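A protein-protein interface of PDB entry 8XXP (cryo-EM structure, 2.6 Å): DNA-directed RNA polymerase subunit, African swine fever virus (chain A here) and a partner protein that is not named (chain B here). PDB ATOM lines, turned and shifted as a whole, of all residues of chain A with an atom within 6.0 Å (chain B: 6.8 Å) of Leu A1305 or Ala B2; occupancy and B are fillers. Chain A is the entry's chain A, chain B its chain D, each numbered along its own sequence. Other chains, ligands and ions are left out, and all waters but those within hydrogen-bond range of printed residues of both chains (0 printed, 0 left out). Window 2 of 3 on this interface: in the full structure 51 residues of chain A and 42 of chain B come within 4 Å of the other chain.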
ATOM      1  N   ILE A1300     -31.315 -24.015 -13.018  1.00  0.00           N
ATOM      2  CA  ILE A1300     -32.266 -23.853 -14.110  1.00  0.00           C
ATOM      3  C   ILE A1300     -31.671 -22.977 -15.199  1.00  0.00           C
ATOM      4  O   ILE A1300     -31.851 -23.239 -16.392  1.00  0.00           O
ATOM      5  CB  ILE A1300     -33.598 -23.287 -13.590  1.00  0.00           C
ATOM      6  CG1 ILE A1300     -34.273 -24.283 -12.651  1.00  0.00           C
ATOM      7  CG2 ILE A1300     -34.520 -22.953 -14.741  1.00  0.00           C
ATOM      8  CD1 ILE A1300     -35.500 -23.737 -11.973  1.00  0.00           C
ATOM      9  N   PHE A1301     -30.952 -21.924 -14.812  1.00  0.00           N
ATOM     10  CA  PHE A1301     -30.335 -21.054 -15.803  1.00  0.00           C
ATOM     11  C   PHE A1301     -29.257 -21.790 -16.583  1.00  0.00           C
ATOM     12  O   PHE A1301     -29.095 -21.572 -17.786  1.00  0.00           O
ATOM     13  CB  PHE A1301     -29.754 -19.816 -15.131  1.00  0.00           C
ATOM     14  CG  PHE A1301     -29.124 -18.854 -16.091  1.00  0.00           C
ATOM     15  CD1 PHE A1301     -29.820 -18.414 -17.201  1.00  0.00           C
ATOM     16  CD2 PHE A1301     -27.834 -18.401 -15.897  1.00  0.00           C
ATOM     17  CE1 PHE A1301     -29.251 -17.533 -18.086  1.00  0.00           C
ATOM     18  CE2 PHE A1301     -27.259 -17.521 -16.784  1.00  0.00           C
ATOM     19  CZ  PHE A1301     -27.968 -17.087 -17.877  1.00  0.00           C
ATOM     20  N   GLY A1302     -28.497 -22.654 -15.910  1.00  0.00           N
ATOM     21  CA  GLY A1302     -27.457 -23.399 -16.600  1.00  0.00           C
ATOM     22  C   GLY A1302     -28.008 -24.369 -17.626  1.00  0.00           C
ATOM     23  O   GLY A1302     -27.484 -24.478 -18.735  1.00  0.00           O
ATOM     24  N   ALA A1303     -29.070 -25.091 -17.267  1.00  0.00           N
ATOM     25  CA  ALA A1303     -29.696 -26.007 -18.211  1.00  0.00           C
ATOM     26  C   ALA A1303     -30.496 -25.265 -19.273  1.00  0.00           C
ATOM     27  O   ALA A1303     -30.745 -25.810 -20.351  1.00  0.00           O
ATOM     28  CB  ALA A1303     -30.586 -26.996 -17.467  1.00  0.00           C
ATOM     29  N   MET A1304     -30.928 -24.037 -18.981  1.00  0.00           N
ATOM     30  CA  MET A1304     -31.600 -23.231 -19.993  1.00  0.00           C
ATOM     31  C   MET A1304     -30.647 -22.841 -21.111  1.00  0.00           C
ATOM     32  O   MET A1304     -31.064 -22.707 -22.265  1.00  0.00           O
ATOM     33  CB  MET A1304     -32.199 -21.978 -19.358  1.00  0.00           C
ATOM     34  CG  MET A1304     -33.692 -22.040 -19.146  1.00  0.00           C
ATOM     35  SD  MET A1304     -34.298 -20.750 -18.043  1.00  0.00           S
ATOM     36  CE  MET A1304     -33.261 -19.370 -18.512  1.00  0.00           C
ATOM     37  N   LEU A1305     -29.371 -22.641 -20.786  1.00  0.00           N
ATOM     38  CA  LEU A1305     -28.376 -22.290 -21.788  1.00  0.00           C
ATOM     39  C   LEU A1305     -27.894 -23.494 -22.583  1.00  0.00           C
ATOM     40  O   LEU A1305     -27.286 -23.316 -23.643  1.00  0.00           O
ATOM     41  CB  LEU A1305     -27.188 -21.602 -21.116  1.00  0.00           C
ATOM     42  CG  LEU A1305     -27.547 -20.341 -20.337  1.00  0.00           C
ATOM     43  CD1 LEU A1305     -26.308 -19.681 -19.781  1.00  0.00           C
ATOM     44  CD2 LEU A1305     -28.307 -19.385 -21.224  1.00  0.00           C
ATOM     45  N   ASP A1306     -28.143 -24.707 -22.103  1.00  0.00           N
ATOM     46  CA  ASP A1306     -27.747 -25.894 -22.846  1.00  0.00           C
ATOM     47  C   ASP A1306     -28.695 -26.118 -24.017  1.00  0.00           C
ATOM     48  O   ASP A1306     -29.918 -26.061 -23.862  1.00  0.00           O
ATOM     49  CB  ASP A1306     -27.730 -27.114 -21.929  1.00  0.00           C
ATOM     50  CG  ASP A1306     -26.918 -28.254 -22.495  1.00  0.00           C
ATOM     51  OD1 ASP A1306     -26.716 -28.290 -23.726  1.00  0.00           O
ATOM     52  OD2 ASP A1306     -26.474 -29.119 -21.711  1.00  0.00           O
ATOM     53  N   ASP A1307     -28.124 -26.362 -25.198  1.00  0.00           N
ATOM     54  CA  ASP A1307     -28.920 -26.569 -26.399  1.00  0.00           C
ATOM     55  C   ASP A1307     -29.497 -27.974 -26.494  1.00  0.00           C
ATOM     56  O   ASP A1307     -30.460 -28.183 -27.237  1.00  0.00           O
ATOM     57  CB  ASP A1307     -28.078 -26.281 -27.643  1.00  0.00           C
ATOM     58  CG  ASP A1307     -28.461 -24.984 -28.318  1.00  0.00           C
ATOM     59  OD1 ASP A1307     -28.937 -24.067 -27.618  1.00  0.00           O
ATOM     60  OD2 ASP A1307     -28.289 -24.881 -29.548  1.00  0.00           O
ATOM     61  N   MET B   1     -24.064 -20.438 -24.725  1.00  0.00           N
ATOM     62  CA  MET B   1     -23.977 -19.741 -23.449  1.00  0.00           C
ATOM     63  C   MET B   1     -25.008 -18.620 -23.356  1.00  0.00           C
ATOM     64  O   MET B   1     -25.946 -18.560 -24.148  1.00  0.00           O
ATOM     65  CB  MET B   1     -22.569 -19.177 -23.238  1.00  0.00           C
ATOM     66  CG  MET B   1     -21.444 -20.148 -23.556  1.00  0.00           C
ATOM     67  SD  MET B   1     -20.165 -20.154 -22.282  1.00  0.00           S
ATOM     68  CE  MET B   1     -21.100 -20.732 -20.867  1.00  0.00           C
ATOM     69  N   ALA B   2     -24.811 -17.726 -22.387  1.00  0.00           N
ATOM     70  CA  ALA B   2     -25.819 -16.716 -22.087  1.00  0.00           C
ATOM     71  C   ALA B   2     -25.984 -15.703 -23.213  1.00  0.00           C
ATOM     72  O   ALA B   2     -27.090 -15.202 -23.430  1.00  0.00           O
ATOM     73  CB  ALA B   2     -25.466 -15.998 -20.787  1.00  0.00           C
ATOM     74  N   MET B   3     -24.907 -15.388 -23.935  1.00  0.00           N
ATOM     75  CA  MET B   3     -24.964 -14.290 -24.895  1.00  0.00           C
ATOM     76  C   MET B   3     -25.799 -14.653 -26.116  1.00  0.00           C
ATOM     77  O   MET B   3     -26.600 -13.841 -26.586  1.00  0.00           O
ATOM     78  CB  MET B   3     -23.554 -13.878 -25.308  1.00  0.00           C
ATOM     79  CG  MET B   3     -23.315 -12.377 -25.275  1.00  0.00           C
ATOM     80  SD  MET B   3     -24.123 -11.572 -23.881  1.00  0.00           S
ATOM     81  CE  MET B   3     -23.123 -12.171 -22.525  1.00  0.00           C
ATOM     82  N   GLN B   4     -25.619 -15.857 -26.659  1.00  0.00           N
ATOM     83  CA  GLN B   4     -26.405 -16.248 -27.826  1.00  0.00           C
ATOM     84  C   GLN B   4     -27.883 -16.383 -27.485  1.00  0.00           C
ATOM     85  O   GLN B   4     -28.747 -15.960 -28.263  1.00  0.00           O
ATOM     86  CB  GLN B   4     -25.875 -17.553 -28.424  1.00  0.00           C
ATOM     87  CG  GLN B   4     -25.287 -18.533 -27.427  1.00  0.00           C
ATOM     88  CD  GLN B   4     -23.808 -18.298 -27.189  1.00  0.00           C
ATOM     89  OE1 GLN B   4     -23.412 -17.284 -26.617  1.00  0.00           O
ATOM     90  NE2 GLN B   4     -22.982 -19.239 -27.633  1.00  0.00           N
ATOM     91  N   LYS B   5     -28.195 -16.978 -26.333  1.00  0.00           N
ATOM     92  CA  LYS B   5     -29.586 -17.082 -25.911  1.00  0.00           C
ATOM     93  C   LYS B   5     -30.192 -15.706 -25.696  1.00  0.00           C
ATOM     94  O   LYS B   5     -31.333 -15.450 -26.094  1.00  0.00           O
ATOM     95  CB  LYS B   5     -29.693 -17.916 -24.637  1.00  0.00           C
ATOM     96  CG  LYS B   5     -29.349 -19.380 -24.815  1.00  0.00           C
ATOM     97  CD  LYS B   5     -30.442 -20.108 -25.568  1.00  0.00           C
ATOM     98  CE  LYS B   5     -30.173 -21.601 -25.616  1.00  0.00           C
ATOM     99  NZ  LYS B   5     -29.057 -21.943 -26.535  1.00  0.00           N
ATOM    100  N   LEU B   6     -29.440 -14.805 -25.069  1.00  0.00           N
ATOM    101  CA  LEU B   6     -29.929 -13.448 -24.871  1.00  0.00           C
ATOM    102  C   LEU B   6     -30.163 -12.757 -26.202  1.00  0.00           C
ATOM    103  O   LEU B   6     -31.173 -12.071 -26.385  1.00  0.00           O
ATOM    104  CB  LEU B   6     -28.936 -12.664 -24.022  1.00  0.00           C
ATOM    105  CG  LEU B   6     -29.486 -11.486 -23.235  1.00  0.00           C
ATOM    106  CD1 LEU B   6     -30.236 -11.983 -22.033  1.00  0.00           C
ATOM    107  CD2 LEU B   6     -28.349 -10.613 -22.803  1.00  0.00           C
ATOM    108  N   PHE B   7     -29.248 -12.946 -27.151  1.00  0.00           N
ATOM    109  CA  PHE B   7     -29.383 -12.322 -28.460  1.00  0.00           C
ATOM    110  C   PHE B   7     -30.612 -12.835 -29.193  1.00  0.00           C
ATOM    111  O   PHE B   7     -31.322 -12.062 -29.844  1.00  0.00           O
ATOM    112  CB  PHE B   7     -28.117 -12.569 -29.281  1.00  0.00           C
ATOM    113  CG  PHE B   7     -28.188 -12.036 -30.681  1.00  0.00           C
ATOM    114  CD1 PHE B   7     -28.047 -10.685 -30.928  1.00  0.00           C
ATOM    115  CD2 PHE B   7     -28.397 -12.885 -31.749  1.00  0.00           C
ATOM    116  CE1 PHE B   7     -28.115 -10.194 -32.209  1.00  0.00           C
ATOM    117  CE2 PHE B   7     -28.469 -12.397 -33.030  1.00  0.00           C
ATOM    118  CZ  PHE B   7     -28.328 -11.051 -33.261  1.00  0.00           C
ATOM    119  N   TYR B  28     -25.194 -12.164 -35.187  1.00  0.00           N
ATOM    120  CA  TYR B  28     -24.778 -12.471 -33.824  1.00  0.00           C
ATOM    121  C   TYR B  28     -23.323 -12.092 -33.589  1.00  0.00           C
ATOM    122  O   TYR B  28     -22.969 -11.599 -32.511  1.00  0.00           O
ATOM    123  CB  TYR B  28     -25.000 -13.955 -33.533  1.00  0.00           C
ATOM    124  CG  TYR B  28     -24.286 -14.458 -32.301  1.00  0.00           C
ATOM    125  CD1 TYR B  28     -24.616 -13.982 -31.041  1.00  0.00           C
ATOM    126  CD2 TYR B  28     -23.289 -15.412 -32.397  1.00  0.00           C
ATOM    127  CE1 TYR B  28     -23.971 -14.440 -29.916  1.00  0.00           C
ATOM    128  CE2 TYR B  28     -22.638 -15.878 -31.275  1.00  0.00           C
ATOM    129  CZ  TYR B  28     -22.982 -15.388 -30.038  1.00  0.00           C
ATOM    130  OH  TYR B  28     -22.333 -15.850 -28.917  1.00  0.00           O
ATOM    131  N   PHE B  31     -23.062  -8.494 -32.907  1.00  0.00           N
ATOM    132  CA  PHE B  31     -23.575  -8.187 -31.575  1.00  0.00           C
ATOM    133  C   PHE B  31     -22.547  -8.504 -30.495  1.00  0.00           C
ATOM    134  O   PHE B  31     -22.296  -7.682 -29.606  1.00  0.00           O
ATOM    135  CB  PHE B  31     -24.874  -8.954 -31.319  1.00  0.00           C
ATOM    136  CG  PHE B  31     -25.060  -9.365 -29.883  1.00  0.00           C
ATOM    137  CD1 PHE B  31     -25.367  -8.434 -28.912  1.00  0.00           C
ATOM    138  CD2 PHE B  31     -24.923 -10.687 -29.506  1.00  0.00           C
ATOM    139  CE1 PHE B  31     -25.530  -8.813 -27.598  1.00  0.00           C
ATOM    140  CE2 PHE B  31     -25.087 -11.065 -28.193  1.00  0.00           C
ATOM    141  CZ  PHE B  31     -25.392 -10.127 -27.240  1.00  0.00           C
ATOM    142  N   ASP B  93     -25.311  -9.127 -15.830  1.00  0.00           N
ATOM    143  CA  ASP B  93     -25.114 -10.375 -15.113  1.00  0.00           C
ATOM    144  C   ASP B  93     -25.811 -10.308 -13.761  1.00  0.00           C
ATOM    145  O   ASP B  93     -25.982  -9.235 -13.181  1.00  0.00           O
ATOM    146  CB  ASP B  93     -23.623 -10.651 -14.924  1.00  0.00           C
ATOM    147  CG  ASP B  93     -23.242 -12.072 -15.277  1.00  0.00           C
ATOM    148  OD1 ASP B  93     -22.233 -12.571 -14.734  1.00  0.00           O
ATOM    149  OD2 ASP B  93     -23.947 -12.690 -16.097  1.00  0.00           O
ATOM    150  N   TYR B 123     -29.559 -11.731 -16.719  1.00  0.00           N
ATOM    151  CA  TYR B 123     -29.602 -12.345 -18.041  1.00  0.00           C
ATOM    152  C   TYR B 123     -30.755 -13.328 -18.169  1.00  0.00           C
ATOM    153  O   TYR B 123     -31.413 -13.381 -19.212  1.00  0.00           O
ATOM    154  CB  TYR B 123     -28.279 -13.048 -18.350  1.00  0.00           C
ATOM    155  CG  TYR B 123     -27.155 -12.116 -18.724  1.00  0.00           C
ATOM    156  CD1 TYR B 123     -27.414 -10.872 -19.279  1.00  0.00           C
ATOM    157  CD2 TYR B 123     -25.833 -12.491 -18.547  1.00  0.00           C
ATOM    158  CE1 TYR B 123     -26.391 -10.023 -19.625  1.00  0.00           C
ATOM    159  CE2 TYR B 123     -24.804 -11.650 -18.895  1.00  0.00           C
ATOM    160  CZ  TYR B 123     -25.089 -10.417 -19.433  1.00  0.00           C
ATOM    161  OH  TYR B 123     -24.062  -9.576 -19.782  1.00  0.00           O
ATOM    162  N   PHE B 126     -34.162 -12.943 -19.978  1.00  0.00           N
ATOM    163  CA  PHE B 126     -34.286 -12.904 -21.428  1.00  0.00           C
ATOM    164  C   PHE B 126     -33.462 -13.988 -22.110  1.00  0.00           C
ATOM    165  O   PHE B 126     -33.124 -13.855 -23.288  1.00  0.00           O
ATOM    166  CB  PHE B 126     -33.885 -11.530 -21.957  1.00  0.00           C
ATOM    167  CG  PHE B 126     -34.437 -10.398 -21.159  1.00  0.00           C
ATOM    168  CD1 PHE B 126     -33.734  -9.877 -20.092  1.00  0.00           C
ATOM    169  CD2 PHE B 126     -35.665  -9.855 -21.470  1.00  0.00           C
ATOM    170  CE1 PHE B 126     -34.247  -8.839 -19.358  1.00  0.00           C
ATOM    171  CE2 PHE B 126     -36.178  -8.817 -20.739  1.00  0.00           C
ATOM    172  CZ  PHE B 126     -35.469  -8.307 -19.684  1.00  0.00           C
ATOM    173  N   CYS B 127     -33.122 -15.054 -21.397  1.00  0.00           N
ATOM    174  CA  CYS B 127     -32.437 -16.188 -21.987  1.00  0.00           C
ATOM    175  C   CYS B 127     -33.393 -17.317 -22.325  1.00  0.00           C
ATOM    176  O   CYS B 127     -32.955 -18.452 -22.533  1.00  0.00           O
ATOM    177  CB  CYS B 127     -31.336 -16.683 -21.053  1.00  0.00           C
ATOM    178  SG  CYS B 127     -29.836 -15.685 -21.104  1.00  0.00           S
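Of the 13 printed residues of chain B, 4 touch a printed residue of chain A. Hydrophobic or aromatic side chains of chain A that line the printed part of chain B: Phe A1301 and Leu A1305. Among the printed residues, 7 pairs touch across the chains. Among the printed residues, Asp or Glu carboxylates within 4 Å of a Lys or Arg side-chain nitrogen of the other chain: Asp A1307 with Lys B5 (2.4 Å).
Of the printed residues of chain B, Phe A1301 touches Ala B2 and Cys B127. Ala A1303 touches none of the printed residues of chain B. Of the printed residues of chain B, Leu A1305 touches Met B1 (3.8 Å), Ala B2 (3.6 Å) and Lys B5 (3.7 Å). Of the printed residues of chain B, Asp A1307 touches Lys B5. Met B3 touches none of the printed residues of chain A. Printed residues of chain A within 4 Å of Lys B5: Met A1304 (3.6 Å), Leu A1305 (3.7 Å) and Asp A1307 (2.4 Å). Of the printed residues of chain A, Cys B127 touches Phe A1301. The nearest printed residue of chain A that does not touch Ala B2 is Asp A1306 (7.7 Å). The nearest printed residue of chain A that does not touch Met B1 is Phe A1301 (6.4 Å).
The side-chain amino group (NZ) of Lys B5 sits close to the side-chain carboxylate (OD1) of Asp A1307 (2.4 Å).
The side-chain sulfur (SG) of Cys B127 is in hydrogen-bond range of the backbone carbonyl oxygen (O) of Tyr B123, at 3.4 Å. The side-chain amide nitrogen of Gln B4 sits close to the backbone NH of Met B1 (3.3 Å). The backbone carbonyl oxygen (O) of Ala B2 lies within hydrogen-bond range of the side-chain sulfur (SG) of Cys B127 (3.6 Å).
CZ of Phe A1301 touches CB of Ala B2, at 3.99 Å. SG of Cys B127 touches CE1 of Phe A1301, at 3.6 Å. Lys B5 touches Met A1304 (CE to O, 3.6 Å). Leu A1305 touches Met B1 (CD2 to O, 3.8 Å). Leu A1305 touches Ala B2 (CD1 to N, 3.6 Å). O of Leu A1305 touches NZ of Lys B5, at 3.7 Å.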
